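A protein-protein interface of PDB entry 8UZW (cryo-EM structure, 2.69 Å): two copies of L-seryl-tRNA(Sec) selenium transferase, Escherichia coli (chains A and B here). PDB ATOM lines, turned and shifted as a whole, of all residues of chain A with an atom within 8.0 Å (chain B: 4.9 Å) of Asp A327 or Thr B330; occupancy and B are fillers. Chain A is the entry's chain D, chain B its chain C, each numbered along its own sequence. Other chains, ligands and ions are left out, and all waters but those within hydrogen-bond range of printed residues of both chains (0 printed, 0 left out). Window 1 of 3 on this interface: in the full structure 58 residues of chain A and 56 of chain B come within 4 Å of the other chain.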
ATOM      1  N   LEU A  80      11.557 -19.079 -23.726  1.00  0.00           N
ATOM      2  CA  LEU A  80      10.542 -18.984 -24.770  1.00  0.00           C
ATOM      3  C   LEU A  80      11.233 -18.961 -26.132  1.00  0.00           C
ATOM      4  O   LEU A  80      11.227 -17.970 -26.865  1.00  0.00           O
ATOM      5  CB  LEU A  80       9.669 -17.755 -24.556  1.00  0.00           C
ATOM      6  CG  LEU A  80       8.744 -17.788 -23.339  1.00  0.00           C
ATOM      7  CD1 LEU A  80       7.950 -16.498 -23.236  1.00  0.00           C
ATOM      8  CD2 LEU A  80       7.825 -18.993 -23.405  1.00  0.00           C
ATOM      9  N   MET A 112       6.758   0.090 -23.325  1.00  0.00           N
ATOM     10  CA  MET A 112       7.679  -0.653 -22.482  1.00  0.00           C
ATOM     11  C   MET A 112       9.005   0.078 -22.307  1.00  0.00           C
ATOM     12  O   MET A 112       9.611   0.012 -21.234  1.00  0.00           O
ATOM     13  CB  MET A 112       7.888  -2.037 -23.103  1.00  0.00           C
ATOM     14  CG  MET A 112       8.922  -2.924 -22.474  1.00  0.00           C
ATOM     15  SD  MET A 112       8.569  -4.615 -22.980  1.00  0.00           S
ATOM     16  CE  MET A 112       9.820  -5.524 -22.092  1.00  0.00           C
ATOM     17  N   LEU A 118      -0.453   5.204 -17.610  1.00  0.00           N
ATOM     18  CA  LEU A 118      -1.184   3.989 -17.268  1.00  0.00           C
ATOM     19  C   LEU A 118      -2.360   4.294 -16.348  1.00  0.00           C
ATOM     20  O   LEU A 118      -3.482   3.830 -16.581  1.00  0.00           O
ATOM     21  CB  LEU A 118      -0.233   2.984 -16.620  1.00  0.00           C
ATOM     22  CG  LEU A 118      -0.796   1.624 -16.214  1.00  0.00           C
ATOM     23  CD1 LEU A 118      -1.495   0.969 -17.387  1.00  0.00           C
ATOM     24  CD2 LEU A 118       0.319   0.742 -15.690  1.00  0.00           C
ATOM     25  N   ARG A 130      -7.392   2.826 -15.056  1.00  0.00           N
ATOM     26  CA  ARG A 130      -6.345   2.169 -15.829  1.00  0.00           C
ATOM     27  C   ARG A 130      -6.786   1.864 -17.258  1.00  0.00           C
ATOM     28  O   ARG A 130      -5.995   2.003 -18.198  1.00  0.00           O
ATOM     29  CB  ARG A 130      -5.917   0.890 -15.111  1.00  0.00           C
ATOM     30  CG  ARG A 130      -4.738   0.192 -15.734  1.00  0.00           C
ATOM     31  CD  ARG A 130      -4.255  -0.957 -14.872  1.00  0.00           C
ATOM     32  NE  ARG A 130      -3.157  -0.551 -14.006  1.00  0.00           N
ATOM     33  CZ  ARG A 130      -2.088  -1.292 -13.760  1.00  0.00           C
ATOM     34  NH1 ARG A 130      -1.935  -2.486 -14.304  1.00  0.00           N
ATOM     35  NH2 ARG A 130      -1.146  -0.820 -12.950  1.00  0.00           N
ATOM     36  N   LEU A 134      -9.433   1.613 -23.323  1.00  0.00           N
ATOM     37  CA  LEU A 134      -9.880   0.326 -23.835  1.00  0.00           C
ATOM     38  C   LEU A 134     -11.380   0.140 -23.658  1.00  0.00           C
ATOM     39  O   LEU A 134     -12.029  -0.469 -24.513  1.00  0.00           O
ATOM     40  CB  LEU A 134      -9.108  -0.790 -23.145  1.00  0.00           C
ATOM     41  CG  LEU A 134      -7.746  -1.040 -23.783  1.00  0.00           C
ATOM     42  CD1 LEU A 134      -6.724  -1.432 -22.744  1.00  0.00           C
ATOM     43  CD2 LEU A 134      -7.872  -2.115 -24.834  1.00  0.00           C
ATOM     44  N   ILE A 149     -10.985  -5.213 -17.761  1.00  0.00           N
ATOM     45  CA  ILE A 149      -9.918  -6.044 -18.302  1.00  0.00           C
ATOM     46  C   ILE A 149      -9.149  -6.664 -17.147  1.00  0.00           C
ATOM     47  O   ILE A 149      -8.719  -5.958 -16.229  1.00  0.00           O
ATOM     48  CB  ILE A 149      -8.977  -5.242 -19.217  1.00  0.00           C
ATOM     49  CG1 ILE A 149      -9.760  -4.675 -20.393  1.00  0.00           C
ATOM     50  CG2 ILE A 149      -7.851  -6.118 -19.726  1.00  0.00           C
ATOM     51  CD1 ILE A 149      -8.990  -3.684 -21.182  1.00  0.00           C
ATOM     52  N   VAL A 150      -8.973  -7.980 -17.203  1.00  0.00           N
ATOM     53  CA  VAL A 150      -8.286  -8.728 -16.160  1.00  0.00           C
ATOM     54  C   VAL A 150      -7.223  -9.623 -16.779  1.00  0.00           C
ATOM     55  O   VAL A 150      -6.997  -9.592 -17.994  1.00  0.00           O
ATOM     56  CB  VAL A 150      -9.276  -9.552 -15.325  1.00  0.00           C
ATOM     57  CG1 VAL A 150     -10.135  -8.645 -14.484  1.00  0.00           C
ATOM     58  CG2 VAL A 150     -10.131 -10.371 -16.232  1.00  0.00           C
ATOM     59  N   ASN A 151      -6.585 -10.438 -15.939  1.00  0.00           N
ATOM     60  CA  ASN A 151      -5.416 -11.207 -16.352  1.00  0.00           C
ATOM     61  C   ASN A 151      -5.732 -12.125 -17.529  1.00  0.00           C
ATOM     62  O   ASN A 151      -5.024 -12.117 -18.541  1.00  0.00           O
ATOM     63  CB  ASN A 151      -4.895 -12.005 -15.159  1.00  0.00           C
ATOM     64  CG  ASN A 151      -3.674 -12.818 -15.489  1.00  0.00           C
ATOM     65  OD1 ASN A 151      -2.865 -12.432 -16.325  1.00  0.00           O
ATOM     66  ND2 ASN A 151      -3.519 -13.944 -14.814  1.00  0.00           N
ATOM     67  N   GLN A 301      -2.864 -12.149 -23.945  1.00  0.00           N
ATOM     68  CA  GLN A 301      -3.636 -12.837 -22.916  1.00  0.00           C
ATOM     69  C   GLN A 301      -4.340 -11.803 -22.051  1.00  0.00           C
ATOM     70  O   GLN A 301      -3.699 -11.098 -21.268  1.00  0.00           O
ATOM     71  CB  GLN A 301      -2.740 -13.731 -22.065  1.00  0.00           C
ATOM     72  CG  GLN A 301      -3.442 -14.286 -20.835  1.00  0.00           C
ATOM     73  CD  GLN A 301      -2.527 -15.085 -19.935  1.00  0.00           C
ATOM     74  OE1 GLN A 301      -2.114 -16.190 -20.275  1.00  0.00           O
ATOM     75  NE2 GLN A 301      -2.213 -14.534 -18.775  1.00  0.00           N
ATOM     76  N   ALA A 302      -5.658 -11.706 -22.194  1.00  0.00           N
ATOM     77  CA  ALA A 302      -6.437 -10.764 -21.412  1.00  0.00           C
ATOM     78  C   ALA A 302      -7.842 -11.310 -21.246  1.00  0.00           C
ATOM     79  O   ALA A 302      -8.316 -12.099 -22.066  1.00  0.00           O
ATOM     80  CB  ALA A 302      -6.478  -9.382 -22.070  1.00  0.00           C
ATOM     81  N   LYS A 321     -10.272  -7.452  -8.048  1.00  0.00           N
ATOM     82  CA  LYS A 321      -9.843  -6.760  -9.258  1.00  0.00           C
ATOM     83  C   LYS A 321      -8.401  -6.289  -9.159  1.00  0.00           C
ATOM     84  O   LYS A 321      -7.682  -6.278 -10.164  1.00  0.00           O
ATOM     85  CB  LYS A 321     -10.778  -5.583  -9.537  1.00  0.00           C
ATOM     86  CG  LYS A 321     -10.303  -4.635 -10.619  1.00  0.00           C
ATOM     87  CD  LYS A 321     -10.257  -5.301 -11.975  1.00  0.00           C
ATOM     88  CE  LYS A 321      -9.902  -4.299 -13.049  1.00  0.00           C
ATOM     89  NZ  LYS A 321      -9.018  -4.892 -14.083  1.00  0.00           N
ATOM     90  N   LEU A 324      -6.300  -9.226 -10.057  1.00  0.00           N
ATOM     91  CA  LEU A 324      -6.500  -9.640 -11.438  1.00  0.00           C
ATOM     92  C   LEU A 324      -6.214  -8.528 -12.435  1.00  0.00           C
ATOM     93  O   LEU A 324      -6.440  -8.718 -13.631  1.00  0.00           O
ATOM     94  CB  LEU A 324      -7.929 -10.150 -11.628  1.00  0.00           C
ATOM     95  CG  LEU A 324      -8.438 -11.092 -10.538  1.00  0.00           C
ATOM     96  CD1 LEU A 324      -9.919 -11.329 -10.684  1.00  0.00           C
ATOM     97  CD2 LEU A 324      -7.688 -12.400 -10.573  1.00  0.00           C
ATOM     98  N   ARG A 325      -5.716  -7.387 -11.972  1.00  0.00           N
ATOM     99  CA  ARG A 325      -5.460  -6.233 -12.821  1.00  0.00           C
ATOM    100  C   ARG A 325      -4.581  -6.608 -14.011  1.00  0.00           C
ATOM    101  O   ARG A 325      -3.837  -7.589 -13.986  1.00  0.00           O
ATOM    102  CB  ARG A 325      -4.791  -5.132 -12.000  1.00  0.00           C
ATOM    103  CG  ARG A 325      -5.372  -3.760 -12.206  1.00  0.00           C
ATOM    104  CD  ARG A 325      -5.098  -2.864 -11.017  1.00  0.00           C
ATOM    105  NE  ARG A 325      -3.682  -2.554 -10.874  1.00  0.00           N
ATOM    106  CZ  ARG A 325      -3.191  -1.703  -9.984  1.00  0.00           C
ATOM    107  NH1 ARG A 325      -3.980  -1.039  -9.158  1.00  0.00           N
ATOM    108  NH2 ARG A 325      -1.878  -1.506  -9.929  1.00  0.00           N
ATOM    109  N   ALA A 326      -4.666  -5.799 -15.063  1.00  0.00           N
ATOM    110  CA  ALA A 326      -3.969  -6.063 -16.314  1.00  0.00           C
ATOM    111  C   ALA A 326      -2.709  -5.216 -16.432  1.00  0.00           C
ATOM    112  O   ALA A 326      -2.702  -4.036 -16.073  1.00  0.00           O
ATOM    113  CB  ALA A 326      -4.883  -5.798 -17.510  1.00  0.00           C
ATOM    114  N   ASP A 327      -1.649  -5.828 -16.956  1.00  0.00           N
ATOM    115  CA  ASP A 327      -0.347  -5.191 -17.083  1.00  0.00           C
ATOM    116  C   ASP A 327      -0.397  -4.073 -18.123  1.00  0.00           C
ATOM    117  O   ASP A 327      -1.342  -3.962 -18.904  1.00  0.00           O
ATOM    118  CB  ASP A 327       0.708  -6.234 -17.460  1.00  0.00           C
ATOM    119  CG  ASP A 327       2.123  -5.686 -17.425  1.00  0.00           C
ATOM    120  OD1 ASP A 327       2.314  -4.547 -16.952  1.00  0.00           O
ATOM    121  OD2 ASP A 327       3.048  -6.401 -17.864  1.00  0.00           O
ATOM    122  N   LYS A 328       0.633  -3.224 -18.114  1.00  0.00           N
ATOM    123  CA  LYS A 328       0.667  -2.117 -19.063  1.00  0.00           C
ATOM    124  C   LYS A 328       0.974  -2.588 -20.482  1.00  0.00           C
ATOM    125  O   LYS A 328       0.438  -2.021 -21.440  1.00  0.00           O
ATOM    126  CB  LYS A 328       1.665  -1.048 -18.606  1.00  0.00           C
ATOM    127  CG  LYS A 328       3.073  -1.183 -19.150  1.00  0.00           C
ATOM    128  CD  LYS A 328       3.897   0.055 -18.842  1.00  0.00           C
ATOM    129  CE  LYS A 328       5.376  -0.276 -18.749  1.00  0.00           C
ATOM    130  NZ  LYS A 328       6.195   0.922 -18.428  1.00  0.00           N
ATOM    131  N   MET A 329       1.814  -3.614 -20.653  1.00  0.00           N
ATOM    132  CA  MET A 329       1.990  -4.160 -21.996  1.00  0.00           C
ATOM    133  C   MET A 329       0.740  -4.896 -22.453  1.00  0.00           C
ATOM    134  O   MET A 329       0.422  -4.902 -23.646  1.00  0.00           O
ATOM    135  CB  MET A 329       3.197  -5.090 -22.084  1.00  0.00           C
ATOM    136  CG  MET A 329       4.379  -4.749 -21.220  1.00  0.00           C
ATOM    137  SD  MET A 329       5.662  -5.977 -21.520  1.00  0.00           S
ATOM    138  CE  MET A 329       5.799  -6.723 -19.913  1.00  0.00           C
ATOM    139  N   THR A 330       0.031  -5.539 -21.528  1.00  0.00           N
ATOM    140  CA  THR A 330      -1.233  -6.165 -21.890  1.00  0.00           C
ATOM    141  C   THR A 330      -2.215  -5.131 -22.416  1.00  0.00           C
ATOM    142  O   THR A 330      -2.849  -5.339 -23.455  1.00  0.00           O
ATOM    143  CB  THR A 330      -1.823  -6.901 -20.688  1.00  0.00           C
ATOM    144  OG1 THR A 330      -0.976  -8.003 -20.344  1.00  0.00           O
ATOM    145  CG2 THR A 330      -3.213  -7.417 -21.009  1.00  0.00           C
ATOM    146  N   LEU A 331      -2.329  -3.994 -21.731  1.00  0.00           N
ATOM    147  CA  LEU A 331      -3.216  -2.935 -22.195  1.00  0.00           C
ATOM    148  C   LEU A 331      -2.735  -2.342 -23.512  1.00  0.00           C
ATOM    149  O   LEU A 331      -3.548  -2.047 -24.393  1.00  0.00           O
ATOM    150  CB  LEU A 331      -3.336  -1.849 -21.131  1.00  0.00           C
ATOM    151  CG  LEU A 331      -3.879  -2.308 -19.782  1.00  0.00           C
ATOM    152  CD1 LEU A 331      -4.035  -1.121 -18.880  1.00  0.00           C
ATOM    153  CD2 LEU A 331      -5.196  -3.030 -19.938  1.00  0.00           C
ATOM    154  N   ALA A 332      -1.424  -2.151 -23.667  1.00  0.00           N
ATOM    155  CA  ALA A 332      -0.898  -1.602 -24.913  1.00  0.00           C
ATOM    156  C   ALA A 332      -1.212  -2.514 -26.093  1.00  0.00           C
ATOM    157  O   ALA A 332      -1.715  -2.062 -27.130  1.00  0.00           O
ATOM    158  CB  ALA A 332       0.610  -1.385 -24.789  1.00  0.00           C
ATOM    159  N   ALA A 333      -0.925  -3.809 -25.945  1.00  0.00           N
ATOM    160  CA  ALA A 333      -1.198  -4.762 -27.010  1.00  0.00           C
ATOM    161  C   ALA A 333      -2.689  -4.867 -27.288  1.00  0.00           C
ATOM    162  O   ALA A 333      -3.103  -4.943 -28.448  1.00  0.00           O
ATOM    163  CB  ALA A 333      -0.623  -6.130 -26.651  1.00  0.00           C
ATOM    164  N   LEU A 334      -3.514  -4.878 -26.238  1.00  0.00           N
ATOM    165  CA  LEU A 334      -4.951  -4.990 -26.447  1.00  0.00           C
ATOM    166  C   LEU A 334      -5.502  -3.770 -27.169  1.00  0.00           C
ATOM    167  O   LEU A 334      -6.338  -3.905 -28.065  1.00  0.00           O
ATOM    168  CB  LEU A 334      -5.662  -5.188 -25.112  1.00  0.00           C
ATOM    169  CG  LEU A 334      -7.057  -5.795 -25.235  1.00  0.00           C
ATOM    170  CD1 LEU A 334      -6.983  -7.159 -25.896  1.00  0.00           C
ATOM    171  CD2 LEU A 334      -7.716  -5.885 -23.877  1.00  0.00           C
ATOM    172  N   ASN B 151       0.121 -12.686 -11.610  1.00  0.00           N
ATOM    173  CA  ASN B 151      -0.166 -11.431 -12.295  1.00  0.00           C
ATOM    174  C   ASN B 151       0.612 -10.266 -11.690  1.00  0.00           C
ATOM    175  O   ASN B 151       1.293  -9.524 -12.405  1.00  0.00           O
ATOM    176  CB  ASN B 151      -1.670 -11.167 -12.252  1.00  0.00           C
ATOM    177  CG  ASN B 151      -2.065  -9.916 -12.987  1.00  0.00           C
ATOM    178  OD1 ASN B 151      -1.455  -9.553 -13.986  1.00  0.00           O
ATOM    179  ND2 ASN B 151      -3.107  -9.260 -12.510  1.00  0.00           N
ATOM    180  N   PRO B 300       8.927  -6.519 -15.686  1.00  0.00           N
ATOM    181  CA  PRO B 300       7.495  -6.399 -15.958  1.00  0.00           C
ATOM    182  C   PRO B 300       6.664  -6.513 -14.685  1.00  0.00           C
ATOM    183  O   PRO B 300       7.147  -6.920 -13.630  1.00  0.00           O
ATOM    184  CB  PRO B 300       7.236  -7.593 -16.878  1.00  0.00           C
ATOM    185  CG  PRO B 300       8.176  -8.623 -16.377  1.00  0.00           C
ATOM    186  CD  PRO B 300       9.413  -7.889 -15.920  1.00  0.00           C
ATOM    187  N   GLN B 301       5.388  -6.157 -14.810  1.00  0.00           N
ATOM    188  CA  GLN B 301       4.454  -6.359 -13.709  1.00  0.00           C
ATOM    189  C   GLN B 301       4.269  -7.852 -13.494  1.00  0.00           C
ATOM    190  O   GLN B 301       3.642  -8.533 -14.311  1.00  0.00           O
ATOM    191  CB  GLN B 301       3.116  -5.687 -13.995  1.00  0.00           C
ATOM    192  CG  GLN B 301       2.028  -6.082 -13.007  1.00  0.00           C
ATOM    193  CD  GLN B 301       0.667  -5.531 -13.365  1.00  0.00           C
ATOM    194  OE1 GLN B 301       0.427  -4.332 -13.274  1.00  0.00           O
ATOM    195  NE2 GLN B 301      -0.236  -6.409 -13.768  1.00  0.00           N
ATOM    196  N   ALA B 302       4.821  -8.369 -12.402  1.00  0.00           N
ATOM    197  CA  ALA B 302       4.712  -9.784 -12.096  1.00  0.00           C
ATOM    198  C   ALA B 302       4.788  -9.965 -10.592  1.00  0.00           C
ATOM    199  O   ALA B 302       5.361  -9.136  -9.883  1.00  0.00           O
ATOM    200  CB  ALA B 302       5.811 -10.596 -12.786  1.00  0.00           C
ATOM    201  N   ALA B 326       0.489 -16.111 -15.542  1.00  0.00           N
ATOM    202  CA  ALA B 326       1.268 -15.036 -16.141  1.00  0.00           C
ATOM    203  C   ALA B 326       1.350 -15.189 -17.656  1.00  0.00           C
ATOM    204  O   ALA B 326       1.517 -16.297 -18.172  1.00  0.00           O
ATOM    205  CB  ALA B 326       2.675 -14.994 -15.550  1.00  0.00           C
ATOM    206  N   ASP B 327       1.249 -14.062 -18.357  1.00  0.00           N
ATOM    207  CA  ASP B 327       1.231 -14.027 -19.812  1.00  0.00           C
ATOM    208  C   ASP B 327       2.609 -14.369 -20.378  1.00  0.00           C
ATOM    209  O   ASP B 327       3.624 -14.305 -19.685  1.00  0.00           O
ATOM    210  CB  ASP B 327       0.777 -12.645 -20.291  1.00  0.00           C
ATOM    211  CG  ASP B 327       0.645 -12.551 -21.802  1.00  0.00           C
ATOM    212  OD1 ASP B 327       0.567 -13.605 -22.468  1.00  0.00           O
ATOM    213  OD2 ASP B 327       0.603 -11.418 -22.325  1.00  0.00           O
ATOM    214  N   LYS B 328       2.634 -14.752 -21.658  1.00  0.00           N
ATOM    215  CA  LYS B 328       3.908 -15.064 -22.300  1.00  0.00           C
ATOM    216  C   LYS B 328       4.774 -13.823 -22.477  1.00  0.00           C
ATOM    217  O   LYS B 328       6.003 -13.919 -22.396  1.00  0.00           O
ATOM    218  CB  LYS B 328       3.680 -15.759 -23.646  1.00  0.00           C
ATOM    219  CG  LYS B 328       3.235 -14.858 -24.784  1.00  0.00           C
ATOM    220  CD  LYS B 328       3.252 -15.599 -26.111  1.00  0.00           C
ATOM    221  CE  LYS B 328       2.755 -14.714 -27.242  1.00  0.00           C
ATOM    222  NZ  LYS B 328       2.743 -15.426 -28.549  1.00  0.00           N
ATOM    223  N   MET B 329       4.169 -12.658 -22.721  1.00  0.00           N
ATOM    224  CA  MET B 329       4.946 -11.423 -22.737  1.00  0.00           C
ATOM    225  C   MET B 329       5.540 -11.137 -21.365  1.00  0.00           C
ATOM    226  O   MET B 329       6.700 -10.723 -21.256  1.00  0.00           O
ATOM    227  CB  MET B 329       4.079 -10.251 -23.193  1.00  0.00           C
ATOM    228  CG  MET B 329       3.613 -10.329 -24.630  1.00  0.00           C
ATOM    229  SD  MET B 329       2.869  -8.782 -25.169  1.00  0.00           S
ATOM    230  CE  MET B 329       1.386  -8.762 -24.180  1.00  0.00           C
ATOM    231  N   THR B 330       4.756 -11.349 -20.308  1.00  0.00           N
ATOM    232  CA  THR B 330       5.261 -11.147 -18.958  1.00  0.00           C
ATOM    233  C   THR B 330       6.418 -12.087 -18.659  1.00  0.00           C
ATOM    234  O   THR B 330       7.443 -11.664 -18.113  1.00  0.00           O
ATOM    235  CB  THR B 330       4.135 -11.344 -17.944  1.00  0.00           C
ATOM    236  OG1 THR B 330       3.144 -10.327 -18.129  1.00  0.00           O
ATOM    237  CG2 THR B 330       4.671 -11.272 -16.527  1.00  0.00           C
ATOM    238  N   LEU B 331       6.281 -13.361 -19.023  1.00  0.00           N
ATOM    239  CA  LEU B 331       7.352 -14.320 -18.776  1.00  0.00           C
ATOM    240  C   LEU B 331       8.596 -13.987 -19.588  1.00  0.00           C
ATOM    241  O   LEU B 331       9.720 -14.102 -19.084  1.00  0.00           O
ATOM    242  CB  LEU B 331       6.873 -15.732 -19.094  1.00  0.00           C
ATOM    243  CG  LEU B 331       5.690 -16.248 -18.281  1.00  0.00           C
ATOM    244  CD1 LEU B 331       5.395 -17.675 -18.665  1.00  0.00           C
ATOM    245  CD2 LEU B 331       5.955 -16.143 -16.798  1.00  0.00           C
ATOM    246  N   ALA B 332       8.423 -13.585 -20.848  1.00  0.00           N
ATOM    247  CA  ALA B 332       9.570 -13.228 -21.676  1.00  0.00           C
ATOM    248  C   ALA B 332      10.310 -12.030 -21.099  1.00  0.00           C
ATOM    249  O   ALA B 332      11.543 -12.038 -20.985  1.00  0.00           O
ATOM    250  CB  ALA B 332       9.112 -12.939 -23.104  1.00  0.00           C
ATOM    251  N   ALA B 333       9.565 -10.991 -20.713  1.00  0.00           N
ATOM    252  CA  ALA B 333      10.189  -9.818 -20.116  1.00  0.00           C
ATOM    253  C   ALA B 333      10.886 -10.175 -18.815  1.00  0.00           C
ATOM    254  O   ALA B 333      11.992  -9.696 -18.545  1.00  0.00           O
ATOM    255  CB  ALA B 333       9.146  -8.728 -19.883  1.00  0.00           C
ATOM    256  N   LEU B 334      10.260 -11.018 -17.994  1.00  0.00           N
ATOM    257  CA  LEU B 334      10.845 -11.359 -16.705  1.00  0.00           C
ATOM    258  C   LEU B 334      12.123 -12.168 -16.871  1.00  0.00           C
ATOM    259  O   LEU B 334      13.107 -11.923 -16.168  1.00  0.00           O
ATOM    260  CB  LEU B 334       9.830 -12.114 -15.853  1.00  0.00           C
ATOM    261  CG  LEU B 334      10.143 -12.141 -14.361  1.00  0.00           C
ATOM    262  CD1 LEU B 334      10.189 -10.729 -13.815  1.00  0.00           C
ATOM    263  CD2 LEU B 334       9.114 -12.967 -13.623  1.00  0.00           C
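Leu A80 touches Lys B328 (CD1 to O, 3.3 Å).
Leu A80 touches Ala B332.
OD1 of Asn A151 touches OD1 of Asn B151 (3.97 Å).
Gln A301 touches Ala B326 (NE2 to C, 3.8 Å).
Gln A301 touches Asp B327.
Arg A325 touches Gln B301.
Gln B301 touches Ala A326.
Asp A327 touches Thr B330 (OD2 to OG1, 3.9 Å).
CE of Met A329 touches CB of Pro B300, 3.5 Å away.
Met A329 touches Ala B333.
Along chain A the printed residues that touch a printed residue of chain B span positions 80 to 329.
Of the 13 printed residues of chain B, 9 touch a printed residue of chain A.
Hydrophobic or aromatic side chains of chain B that line the printed part of chain A: Pro B300, Ala B332 and Ala B333.
Among the printed residues, no Asp or Glu carboxylate lies within 4 Å of a Lys or Arg side-chain nitrogen of the other chain.
Of the printed residues of chain B, Arg A325 touches Asn B151 and Gln B301.
Of the printed residues of chain B, Ala A326 touches Gln B301.
Of chain B, only Gln B301 (3.3 Å) and Thr B330 (3.9 Å) come within 4 Å of Asp A327.
Leu A331 touches none of the printed residues of chain B.
Printed residues of chain A within 4 Å of Asn B151: Asn A151, Leu A324 and Arg A325.
The side-chain amide oxygen (OD1) of Asn B151 is in hydrogen-bond range of the side-chain amide nitrogen (NE2) of Gln B301 (3.4 Å).
NH1 of Arg A130 sits at hydrogen-bond distance from O of Ala A326, 2.5 Å away.
OD1 of Asn A151 lies within hydrogen-bond range of NE2 of Gln A301.
O of Leu A324 lies within hydrogen-bond range of N of Asn A151.
The side-chain amide oxygen (OD1) of Asn B151 sits close to the backbone carbonyl oxygen (O) of Arg A325 (3.1 Å).
NH1 of Arg A130 lies within hydrogen-bond range of OE1 of Gln B301 (3.2 Å).
Asn B151 touches its own counterpart, Asn A151.
Gln A301 touches Ala B326, and with the chains exchanged Ala A326 touches Gln B301.
Asp A327 touches Thr B330, but with the chains exchanged Thr A330 does not touch Asp B327 (4.3 Å).
Met A329 touches Ala B333, but with the chains exchanged Ala A333 does not touch Met B329 (4.1 Å).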
